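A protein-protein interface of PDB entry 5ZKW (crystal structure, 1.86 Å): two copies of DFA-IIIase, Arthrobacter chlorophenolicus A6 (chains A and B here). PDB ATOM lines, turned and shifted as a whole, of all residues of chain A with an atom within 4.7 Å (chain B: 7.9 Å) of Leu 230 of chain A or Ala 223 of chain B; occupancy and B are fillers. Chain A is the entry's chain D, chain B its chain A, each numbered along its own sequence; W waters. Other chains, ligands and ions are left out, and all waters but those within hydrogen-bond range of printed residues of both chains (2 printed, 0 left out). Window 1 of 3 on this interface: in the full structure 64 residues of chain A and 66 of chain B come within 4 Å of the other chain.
The backbone NH of Ser 178 of chain B sits at hydrogen-bond distance from the backbone carbonyl oxygen of Asp 199 of chain B (3.0 Å).
N of Ala 200 of chain B lies within hydrogen-bond range of O of Gln 222 of chain B, at 2.9 Å.
OG of Ser 202 of chain B lies within hydrogen-bond range of NZ of Lys 225 of chain B (3.0 Å).
O of Gln 222 of chain B is in hydrogen-bond range of OG of Ser 224 of chain B (3.0 Å).
N of Ile 208 of chain A lies within hydrogen-bond range of O of Leu 230 of chain A (2.8 Å).
O of Asn 254 of chain A lies within hydrogen-bond range of N of Val 231 of chain A (3.1 Å).
O of Ser 224 of chain B is in hydrogen-bond range of ND2 of Asn 254 of chain A.
The side-chain carboxylate (OD2) of Asp 228 of chain A is in salt-bridge range of the side-chain amino group (NZ) of Lys 225 of chain B.
The backbone carbonyl oxygen (O) of Gly 247 of chain B lies within hydrogen-bond range of the side-chain amide nitrogen (ND2) of Asn 254 of chain A (2.9 Å).
Leu 230 of chain A touches three residues of chain B.
Of chain A, only Leu 230, Asn 254 and Arg 277 come within 4 Å of Ala 223 of chain B.
Of the printed residues of chain B, Asn 229 of chain A touches Lys 225.
Printed residues of chain A within 4 Å of Gly 247 of chain B: Asn 254 and Arg 277.
Of the printed residues of chain A, Ala 200 of chain B touches Phe 207 (3.6 Å) and Leu 230 (3.5 Å).
The nearest residue of chain A that does not touch Ala 223 of chain B is Phe 256 of chain A (4.2 Å).
The nearest printed residue of chain A that does not touch Arg 180 of chain B is Asn 206 of chain A (4.1 Å).
Water W1 lies within hydrogen-bond range of the backbone carbonyl oxygen of Arg 270 of chain B (2.7 Å) and the guanidinium group of Arg 277 of chain A (2.8 Å).
Water W2 lies within hydrogen-bond range of NZ of Lys 225 of chain B (3.0 Å), O of Asn 206 of chain A (3.3 Å) and O of Asp 228 of chain A (3.4 Å).
CD2 of Phe 207 of chain A touches OG of Ser 178 of chain B (3.2 Å).
NH2 of Arg 180 of chain B touches N of Phe 207 of chain A, 3.7 Å away.
Ala 200 of chain B touches Phe 207 of chain A (CB to CE2, 3.6 Å).
Asn 229 of chain A touches Lys 225 of chain B.
Leu 230 of chain A touches Ala 200 of chain B (CD1 to O, 3.5 Å).
CD2 of Leu 230 of chain A touches O of Ala 223 of chain B, at 3.2 Å.
Lys 225 of chain B touches Leu 230 of chain A (CE to CG, 3.6 Å).
Asn 254 of chain A touches Ala 223 of chain B (ND2 to C, 3.5 Å).
Ala 223 of chain B touches Arg 277 of chain A (CB to NH1, 3.7 Å).
Arg 277 of chain A touches Gly 247 of chain B.
Of the 22 printed residues of chain B, 7 touch a printed residue of chain A.
Hydrophobic or aromatic side chains of chain B within 4 Å of the printed part of chain A: Ala 200 and Ala 223.
Of the 11 printed residues of chain A, 6 touch a printed residue of chain B.
Among the printed residues, 13 pairs touch across the chains.
Among the printed residues, Asp or Glu carboxylates within 4 Å of a Lys or Arg side-chain nitrogen of the other chain: Asp 228 of chain A with Lys 225 of chain B.
No position is printed for both chains.
Of the 13 pairs that touch across the chains among the printed residues, none has its exchanged pair printed and touching as well.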
ATOM      1  N   ASN A 206      -2.722  11.053 -16.507  1.00  0.00           N
ATOM      2  CA  ASN A 206      -1.297  11.341 -16.613  1.00  0.00           C
ATOM      3  C   ASN A 206      -0.672  11.530 -15.242  1.00  0.00           C
ATOM      4  O   ASN A 206      -1.368  11.769 -14.251  1.00  0.00           O
ATOM      5  CB  ASN A 206      -1.070  12.595 -17.455  1.00  0.00           C
ATOM      6  CG  ASN A 206      -1.726  12.503 -18.816  1.00  0.00           C
ATOM      7  OD1 ASN A 206      -1.183  11.890 -19.738  1.00  0.00           O
ATOM      8  ND2 ASN A 206      -2.907  13.102 -18.946  1.00  0.00           N
ATOM      9  N   PHE A 207       0.656  11.432 -15.212  1.00  0.00           N
ATOM     10  CA  PHE A 207       1.458  11.718 -14.031  1.00  0.00           C
ATOM     11  C   PHE A 207       2.316  12.925 -14.395  1.00  0.00           C
ATOM     12  O   PHE A 207       3.227  12.810 -15.211  1.00  0.00           O
ATOM     13  CB  PHE A 207       2.314  10.509 -13.651  1.00  0.00           C
ATOM     14  CG  PHE A 207       2.824  10.561 -12.245  1.00  0.00           C
ATOM     15  CD1 PHE A 207       3.942  11.335 -11.928  1.00  0.00           C
ATOM     16  CD2 PHE A 207       2.182   9.854 -11.225  1.00  0.00           C
ATOM     17  CE1 PHE A 207       4.406  11.408 -10.622  1.00  0.00           C
ATOM     18  CE2 PHE A 207       2.659   9.909  -9.923  1.00  0.00           C
ATOM     19  CZ  PHE A 207       3.760  10.705  -9.621  1.00  0.00           C
ATOM     20  N   ILE A 208       1.963  14.085 -13.847  1.00  0.00           N
ATOM     21  CA  ILE A 208       2.568  15.358 -14.253  1.00  0.00           C
ATOM     22  C   ILE A 208       3.123  16.013 -12.998  1.00  0.00           C
ATOM     23  O   ILE A 208       2.381  16.669 -12.225  1.00  0.00           O
ATOM     24  CB  ILE A 208       1.555  16.284 -14.960  1.00  0.00           C
ATOM     25  CG1 ILE A 208       0.606  15.473 -15.870  1.00  0.00           C
ATOM     26  CG2 ILE A 208       2.300  17.369 -15.740  1.00  0.00           C
ATOM     27  CD1 ILE A 208      -0.408  16.299 -16.630  1.00  0.00           C
ATOM     28  N   ASP A 228      -8.588  12.452 -13.708  1.00  0.00           N
ATOM     29  CA  ASP A 228      -7.847  11.286 -13.225  1.00  0.00           C
ATOM     30  C   ASP A 228      -6.327  11.454 -13.311  1.00  0.00           C
ATOM     31  O   ASP A 228      -5.621  10.480 -13.471  1.00  0.00           O
ATOM     32  CB  ASP A 228      -8.332  10.008 -13.957  1.00  0.00           C
ATOM     33  CG  ASP A 228      -8.789   8.918 -12.994  1.00  0.00           C
ATOM     34  OD1 ASP A 228     -10.010   8.661 -12.952  1.00  0.00           O
ATOM     35  OD2 ASP A 228      -7.956   8.328 -12.273  1.00  0.00           O
ATOM     36  N   ASN A 229      -5.834  12.682 -13.169  1.00  0.00           N
ATOM     37  CA  ASN A 229      -4.390  12.946 -13.216  1.00  0.00           C
ATOM     38  C   ASN A 229      -3.800  13.016 -11.817  1.00  0.00           C
ATOM     39  O   ASN A 229      -4.495  13.337 -10.848  1.00  0.00           O
ATOM     40  CB  ASN A 229      -4.114  14.255 -13.949  1.00  0.00           C
ATOM     41  CG  ASN A 229      -4.612  14.227 -15.377  1.00  0.00           C
ATOM     42  OD1 ASN A 229      -3.983  13.627 -16.239  1.00  0.00           O
ATOM     43  ND2 ASN A 229      -5.739  14.860 -15.627  1.00  0.00           N
ATOM     44  N   LEU A 230      -2.515  12.716 -11.739  1.00  0.00           N
ATOM     45  CA  LEU A 230      -1.698  12.947 -10.552  1.00  0.00           C
ATOM     46  C   LEU A 230      -0.793  14.134 -10.902  1.00  0.00           C
ATOM     47  O   LEU A 230      -0.033  14.055 -11.876  1.00  0.00           O
ATOM     48  CB  LEU A 230      -0.892  11.692 -10.218  1.00  0.00           C
ATOM     49  CG  LEU A 230      -1.671  10.690  -9.356  1.00  0.00           C
ATOM     50  CD1 LEU A 230      -1.183   9.260  -9.556  1.00  0.00           C
ATOM     51  CD2 LEU A 230      -1.606  11.077  -7.890  1.00  0.00           C
ATOM     52  N   VAL A 231      -0.897  15.228 -10.138  1.00  0.00           N
ATOM     53  CA  VAL A 231      -0.322  16.511 -10.537  1.00  0.00           C
ATOM     54  C   VAL A 231       0.408  17.166  -9.364  1.00  0.00           C
ATOM     55  O   VAL A 231      -0.136  17.259  -8.259  1.00  0.00           O
ATOM     56  CB  VAL A 231      -1.403  17.487 -11.061  1.00  0.00           C
ATOM     57  CG1 VAL A 231      -0.755  18.749 -11.634  1.00  0.00           C
ATOM     58  CG2 VAL A 231      -2.289  16.826 -12.121  1.00  0.00           C
ATOM     59  N   GLY A 232       1.630  17.631  -9.617  1.00  0.00           N
ATOM     60  CA  GLY A 232       2.390  18.384  -8.623  1.00  0.00           C
ATOM     61  C   GLY A 232       3.280  19.385  -9.322  1.00  0.00           C
ATOM     62  O   GLY A 232       4.097  19.003 -10.148  1.00  0.00           O
ATOM     63  N   ASN A 254      -5.807  14.017  -8.355  1.00  0.00           N
ATOM     64  CA  ASN A 254      -5.115  14.065  -7.087  1.00  0.00           C
ATOM     65  C   ASN A 254      -3.953  15.040  -7.303  1.00  0.00           C
ATOM     66  O   ASN A 254      -2.952  14.707  -7.939  1.00  0.00           O
ATOM     67  CB  ASN A 254      -4.650  12.667  -6.664  1.00  0.00           C
ATOM     68  CG  ASN A 254      -4.229  12.605  -5.215  1.00  0.00           C
ATOM     69  OD1 ASN A 254      -3.533  13.510  -4.733  1.00  0.00           O
ATOM     70  ND2 ASN A 254      -4.642  11.543  -4.502  1.00  0.00           N
ATOM     71  N   PHE A 256      -1.155  17.331  -5.676  1.00  0.00           N
ATOM     72  CA  PHE A 256      -0.322  17.428  -4.469  1.00  0.00           C
ATOM     73  C   PHE A 256       0.630  18.619  -4.646  1.00  0.00           C
ATOM     74  O   PHE A 256       0.636  19.258  -5.708  1.00  0.00           O
ATOM     75  CB  PHE A 256       0.384  16.091  -4.173  1.00  0.00           C
ATOM     76  CG  PHE A 256       0.988  15.432  -5.380  1.00  0.00           C
ATOM     77  CD1 PHE A 256       2.247  15.796  -5.824  1.00  0.00           C
ATOM     78  CD2 PHE A 256       0.294  14.452  -6.077  1.00  0.00           C
ATOM     79  CE1 PHE A 256       2.808  15.192  -6.941  1.00  0.00           C
ATOM     80  CE2 PHE A 256       0.844  13.846  -7.195  1.00  0.00           C
ATOM     81  CZ  PHE A 256       2.106  14.207  -7.625  1.00  0.00           C
ATOM     82  N   ARG A 277      -9.021  15.655  -5.136  1.00  0.00           N
ATOM     83  CA  ARG A 277      -8.278  15.748  -3.893  1.00  0.00           C
ATOM     84  C   ARG A 277      -7.157  16.758  -4.132  1.00  0.00           C
ATOM     85  O   ARG A 277      -6.370  16.605  -5.080  1.00  0.00           O
ATOM     86  CB  ARG A 277      -7.775  14.376  -3.474  1.00  0.00           C
ATOM     87  CG  ARG A 277      -7.014  14.366  -2.160  1.00  0.00           C
ATOM     88  CD  ARG A 277      -5.539  14.597  -2.379  1.00  0.00           C
ATOM     89  NE  ARG A 277      -4.797  14.769  -1.137  1.00  0.00           N
ATOM     90  CZ  ARG A 277      -3.473  14.626  -1.000  1.00  0.00           C
ATOM     91  NH1 ARG A 277      -2.685  14.270  -2.019  1.00  0.00           N
ATOM     92  NH2 ARG A 277      -2.931  14.805   0.201  1.00  0.00           N
ATOM     93  N   ASP B 177       6.626   4.228  -5.747  1.00  0.00           N
ATOM     94  CA  ASP B 177       6.187   5.534  -6.197  1.00  0.00           C
ATOM     95  C   ASP B 177       5.695   5.452  -7.643  1.00  0.00           C
ATOM     96  O   ASP B 177       6.336   4.804  -8.482  1.00  0.00           O
ATOM     97  CB  ASP B 177       7.349   6.528  -6.083  1.00  0.00           C
ATOM     98  CG  ASP B 177       6.920   7.975  -6.300  1.00  0.00           C
ATOM     99  OD1 ASP B 177       5.773   8.354  -5.972  1.00  0.00           O
ATOM    100  OD2 ASP B 177       7.738   8.744  -6.827  1.00  0.00           O
ATOM    101  N   SER B 178       4.559   6.076  -7.930  1.00  0.00           N
ATOM    102  CA  SER B 178       4.068   6.242  -9.313  1.00  0.00           C
ATOM    103  C   SER B 178       3.734   4.920 -10.048  1.00  0.00           C
ATOM    104  O   SER B 178       3.819   4.854 -11.271  1.00  0.00           O
ATOM    105  CB  SER B 178       5.073   7.082 -10.130  1.00  0.00           C
ATOM    106  OG  SER B 178       4.485   7.674 -11.284  1.00  0.00           O
ATOM    107  N   PHE B 179       3.392   3.876  -9.292  1.00  0.00           N
ATOM    108  CA  PHE B 179       2.958   2.591  -9.850  1.00  0.00           C
ATOM    109  C   PHE B 179       1.577   2.738 -10.481  1.00  0.00           C
ATOM    110  O   PHE B 179       0.787   3.620 -10.083  1.00  0.00           O
ATOM    111  CB  PHE B 179       2.873   1.501  -8.766  1.00  0.00           C
ATOM    112  CG  PHE B 179       4.160   0.769  -8.506  1.00  0.00           C
ATOM    113  CD1 PHE B 179       5.400   1.394  -8.630  1.00  0.00           C
ATOM    114  CD2 PHE B 179       4.120  -0.562  -8.109  1.00  0.00           C
ATOM    115  CE1 PHE B 179       6.573   0.680  -8.392  1.00  0.00           C
ATOM    116  CE2 PHE B 179       5.278  -1.269  -7.854  1.00  0.00           C
ATOM    117  CZ  PHE B 179       6.509  -0.644  -7.994  1.00  0.00           C
ATOM    118  N   ARG B 180       1.311   1.881 -11.466  1.00  0.00           N
ATOM    119  CA  ARG B 180      -0.002   1.813 -12.119  1.00  0.00           C
ATOM    120  C   ARG B 180      -0.465   0.395 -12.326  1.00  0.00           C
ATOM    121  O   ARG B 180       0.305  -0.450 -12.765  1.00  0.00           O
ATOM    122  CB  ARG B 180       0.058   2.432 -13.500  1.00  0.00           C
ATOM    123  CG  ARG B 180       0.230   3.905 -13.497  1.00  0.00           C
ATOM    124  CD  ARG B 180       0.365   4.359 -14.928  1.00  0.00           C
ATOM    125  NE  ARG B 180       0.459   5.801 -15.008  1.00  0.00           N
ATOM    126  CZ  ARG B 180       0.753   6.462 -16.124  1.00  0.00           C
ATOM    127  NH1 ARG B 180       0.990   5.793 -17.265  1.00  0.00           N
ATOM    128  NH2 ARG B 180       0.782   7.794 -16.099  1.00  0.00           N
ATOM    129  N   ALA B 198       2.519   2.513  -0.567  1.00  0.00           N
ATOM    130  CA  ALA B 198       2.347   3.158  -1.867  1.00  0.00           C
ATOM    131  C   ALA B 198       2.309   4.677  -1.785  1.00  0.00           C
ATOM    132  O   ALA B 198       1.576   5.240  -0.972  1.00  0.00           O
ATOM    133  CB  ALA B 198       1.067   2.648  -2.532  1.00  0.00           C
ATOM    134  N   ASP B 199       3.050   5.321  -2.682  1.00  0.00           N
ATOM    135  CA  ASP B 199       3.004   6.754  -2.902  1.00  0.00           C
ATOM    136  C   ASP B 199       2.588   7.019  -4.346  1.00  0.00           C
ATOM    137  O   ASP B 199       3.186   6.483  -5.281  1.00  0.00           O
ATOM    138  CB  ASP B 199       4.382   7.377  -2.621  1.00  0.00           C
ATOM    139  CG  ASP B 199       4.389   8.911  -2.701  1.00  0.00           C
ATOM    140  OD1 ASP B 199       3.329   9.549  -2.929  1.00  0.00           O
ATOM    141  OD2 ASP B 199       5.484   9.507  -2.513  1.00  0.00           O
ATOM    142  N   ALA B 200       1.573   7.861  -4.521  1.00  0.00           N
ATOM    143  CA  ALA B 200       1.159   8.324  -5.842  1.00  0.00           C
ATOM    144  C   ALA B 200       0.844   7.162  -6.811  1.00  0.00           C
ATOM    145  O   ALA B 200       1.170   7.204  -7.987  1.00  0.00           O
ATOM    146  CB  ALA B 200       2.197   9.285  -6.411  1.00  0.00           C
ATOM    147  N   LEU B 201       0.197   6.141  -6.256  1.00  0.00           N
ATOM    148  CA  LEU B 201      -0.289   4.962  -6.969  1.00  0.00           C
ATOM    149  C   LEU B 201      -1.622   5.247  -7.673  1.00  0.00           C
ATOM    150  O   LEU B 201      -2.465   6.000  -7.157  1.00  0.00           O
ATOM    151  CB  LEU B 201      -0.496   3.818  -5.962  1.00  0.00           C
ATOM    152  CG  LEU B 201      -1.344   2.594  -6.339  1.00  0.00           C
ATOM    153  CD1 LEU B 201      -0.589   1.689  -7.296  1.00  0.00           C
ATOM    154  CD2 LEU B 201      -1.770   1.830  -5.102  1.00  0.00           C
ATOM    155  N   SER B 202      -1.823   4.617  -8.828  1.00  0.00           N
ATOM    156  CA  SER B 202      -3.100   4.696  -9.533  1.00  0.00           C
ATOM    157  C   SER B 202      -3.567   3.283  -9.849  1.00  0.00           C
ATOM    158  O   SER B 202      -2.865   2.535 -10.519  1.00  0.00           O
ATOM    159  CB  SER B 202      -2.947   5.501 -10.817  1.00  0.00           C
ATOM    160  OG  SER B 202      -4.188   5.596 -11.495  1.00  0.00           O
ATOM    161  N   ILE B 203      -4.727   2.899  -9.315  1.00  0.00           N
ATOM    162  CA  ILE B 203      -5.373   1.657  -9.673  1.00  0.00           C
ATOM    163  C   ILE B 203      -6.638   2.086 -10.427  1.00  0.00           C
ATOM    164  O   ILE B 203      -7.592   2.559  -9.800  1.00  0.00           O
ATOM    165  CB  ILE B 203      -5.732   0.811  -8.434  1.00  0.00           C
ATOM    166  CG1 ILE B 203      -4.467   0.371  -7.700  1.00  0.00           C
ATOM    167  CG2 ILE B 203      -6.541  -0.411  -8.850  1.00  0.00           C
ATOM    168  CD1 ILE B 203      -4.724  -0.103  -6.282  1.00  0.00           C
ATOM    169  N   GLY B 221       0.619   4.864   3.181  1.00  0.00           N
ATOM    170  CA  GLY B 221       0.724   5.423   1.846  1.00  0.00           C
ATOM    171  C   GLY B 221       0.248   6.853   1.754  1.00  0.00           C
ATOM    172  O   GLY B 221      -0.239   7.434   2.730  1.00  0.00           O
ATOM    173  N   GLN B 222       0.423   7.439   0.577  1.00  0.00           N
ATOM    174  CA  GLN B 222      -0.053   8.788   0.342  1.00  0.00           C
ATOM    175  C   GLN B 222      -0.343   9.070  -1.109  1.00  0.00           C
ATOM    176  O   GLN B 222       0.203   8.413  -1.987  1.00  0.00           O
ATOM    177  CB  GLN B 222       0.966   9.817   0.847  1.00  0.00           C
ATOM    178  CG  GLN B 222       2.359   9.642   0.287  1.00  0.00           C
ATOM    179  CD  GLN B 222       3.247  10.868   0.469  1.00  0.00           C
ATOM    180  OE1 GLN B 222       2.827  11.885   1.046  1.00  0.00           O
ATOM    181  NE2 GLN B 222       4.482  10.785  -0.040  1.00  0.00           N
ATOM    182  N   ALA B 223      -1.188  10.078  -1.322  1.00  0.00           N
ATOM    183  CA  ALA B 223      -1.456  10.696  -2.614  1.00  0.00           C
ATOM    184  C   ALA B 223      -1.800   9.722  -3.743  1.00  0.00           C
ATOM    185  O   ALA B 223      -1.442   9.951  -4.898  1.00  0.00           O
ATOM    186  CB  ALA B 223      -0.298  11.598  -3.019  1.00  0.00           C
ATOM    187  N   SER B 224      -2.539   8.675  -3.395  1.00  0.00           N
ATOM    188  CA  SER B 224      -2.878   7.601  -4.321  1.00  0.00           C
ATOM    189  C   SER B 224      -4.347   7.687  -4.726  1.00  0.00           C
ATOM    190  O   SER B 224      -5.119   8.484  -4.172  1.00  0.00           O
ATOM    191  CB  SER B 224      -2.561   6.245  -3.687  1.00  0.00           C
ATOM    192  OG  SER B 224      -1.159   6.130  -3.416  1.00  0.00           O
ATOM    193  N   LYS B 225      -4.721   6.895  -5.720  1.00  0.00           N
ATOM    194  CA  LYS B 225      -6.092   6.912  -6.213  1.00  0.00           C
ATOM    195  C   LYS B 225      -6.551   5.570  -6.749  1.00  0.00           C
ATOM    196  O   LYS B 225      -5.781   4.845  -7.381  1.00  0.00           O
ATOM    197  CB  LYS B 225      -6.313   8.042  -7.235  1.00  0.00           C
ATOM    198  CG  LYS B 225      -5.507   8.003  -8.501  1.00  0.00           C
ATOM    199  CD  LYS B 225      -5.810   9.272  -9.326  1.00  0.00           C
ATOM    200  CE  LYS B 225      -4.875   9.394 -10.504  1.00  0.00           C
ATOM    201  NZ  LYS B 225      -5.163   8.405 -11.581  1.00  0.00           N
ATOM    202  N   HIS B 245      -3.221   5.537   5.145  1.00  0.00           N
ATOM    203  CA  HIS B 245      -3.075   6.319   3.944  1.00  0.00           C
ATOM    204  C   HIS B 245      -3.543   7.739   4.240  1.00  0.00           C
ATOM    205  O   HIS B 245      -4.474   7.945   5.018  1.00  0.00           O
ATOM    206  CB  HIS B 245      -3.896   5.724   2.781  1.00  0.00           C
ATOM    207  CG  HIS B 245      -3.085   4.888   1.845  1.00  0.00           C
ATOM    208  ND1 HIS B 245      -2.731   5.318   0.582  1.00  0.00           N
ATOM    209  CD2 HIS B 245      -2.537   3.654   1.993  1.00  0.00           C
ATOM    210  CE1 HIS B 245      -2.008   4.381  -0.009  1.00  0.00           C
ATOM    211  NE2 HIS B 245      -1.867   3.366   0.829  1.00  0.00           N
ATOM    212  N   GLY B 246      -2.860   8.702   3.633  1.00  0.00           N
ATOM    213  CA  GLY B 246      -3.248  10.108   3.658  1.00  0.00           C
ATOM    214  C   GLY B 246      -3.484  10.523   2.226  1.00  0.00           C
ATOM    215  O   GLY B 246      -2.752  10.105   1.342  1.00  0.00           O
ATOM    216  N   GLY B 247      -4.495  11.349   1.979  1.00  0.00           N
ATOM    217  CA  GLY B 247      -4.680  11.902   0.632  1.00  0.00           C
ATOM    218  C   GLY B 247      -5.074  10.890  -0.431  1.00  0.00           C
ATOM    219  O   GLY B 247      -4.734  11.065  -1.600  1.00  0.00           O
ATOM    220  N   LEU B 248      -5.759   9.829  -0.016  1.00  0.00           N
ATOM    221  CA  LEU B 248      -6.278   8.796  -0.930  1.00  0.00           C
ATOM    222  C   LEU B 248      -7.597   9.270  -1.568  1.00  0.00           C
ATOM    223  O   LEU B 248      -8.436   9.856  -0.884  1.00  0.00           O
ATOM    224  CB  LEU B 248      -6.487   7.477  -0.175  1.00  0.00           C
ATOM    225  CG  LEU B 248      -7.068   6.267  -0.941  1.00  0.00           C
ATOM    226  CD1 LEU B 248      -6.152   5.790  -2.056  1.00  0.00           C
ATOM    227  CD2 LEU B 248      -7.395   5.124   0.009  1.00  0.00           C
ATOM    228  N   LEU B 249      -7.754   9.040  -2.875  1.00  0.00           N
ATOM    229  CA  LEU B 249      -8.982   9.388  -3.605  1.00  0.00           C
ATOM    230  C   LEU B 249      -9.586   8.111  -4.137  1.00  0.00           C
ATOM    231  O   LEU B 249      -8.975   7.452  -4.955  1.00  0.00           O
ATOM    232  CB  LEU B 249      -8.678  10.337  -4.770  1.00  0.00           C
ATOM    233  CG  LEU B 249      -9.841  10.729  -5.695  1.00  0.00           C
ATOM    234  CD1 LEU B 249     -10.951  11.439  -4.929  1.00  0.00           C
ATOM    235  CD2 LEU B 249      -9.299  11.607  -6.819  1.00  0.00           C
ATOM    236  N   ARG B 270      -7.637  12.400   5.811  1.00  0.00           N
ATOM    237  CA  ARG B 270      -7.523  13.445   4.783  1.00  0.00           C
ATOM    238  C   ARG B 270      -7.676  12.868   3.376  1.00  0.00           C
ATOM    239  O   ARG B 270      -6.931  13.215   2.443  1.00  0.00           O
ATOM    240  CB  ARG B 270      -6.200  14.202   4.984  1.00  0.00           C
ATOM    241  CG  ARG B 270      -6.246  14.998   6.276  1.00  0.00           C
ATOM    242  CD  ARG B 270      -4.913  15.535   6.752  1.00  0.00           C
ATOM    243  NE  ARG B 270      -5.120  16.157   8.061  1.00  0.00           N
ATOM    244  CZ  ARG B 270      -4.180  16.354   8.989  1.00  0.00           C
ATOM    245  NH1 ARG B 270      -2.915  16.011   8.776  1.00  0.00           N
ATOM    246  NH2 ARG B 270      -4.517  16.909  10.156  1.00  0.00           N
ATOM    247  N   SER B 271      -8.673  11.990   3.243  1.00  0.00           N
ATOM    248  CA  SER B 271      -8.920  11.253   2.020  1.00  0.00           C
ATOM    249  C   SER B 271     -10.375  11.460   1.603  1.00  0.00           C
ATOM    250  O   SER B 271     -11.166  12.058   2.338  1.00  0.00           O
ATOM    251  CB  SER B 271      -8.628   9.762   2.248  1.00  0.00           C
ATOM    252  OG  SER B 271      -7.236   9.545   2.535  1.00  0.00           O
HETATM  253  O   HOH W   1      -5.210  15.264   1.816  1.00  0.00           O
HETATM  254  O   HOH W   2      -2.644   8.953 -13.207  1.00  0.00           O
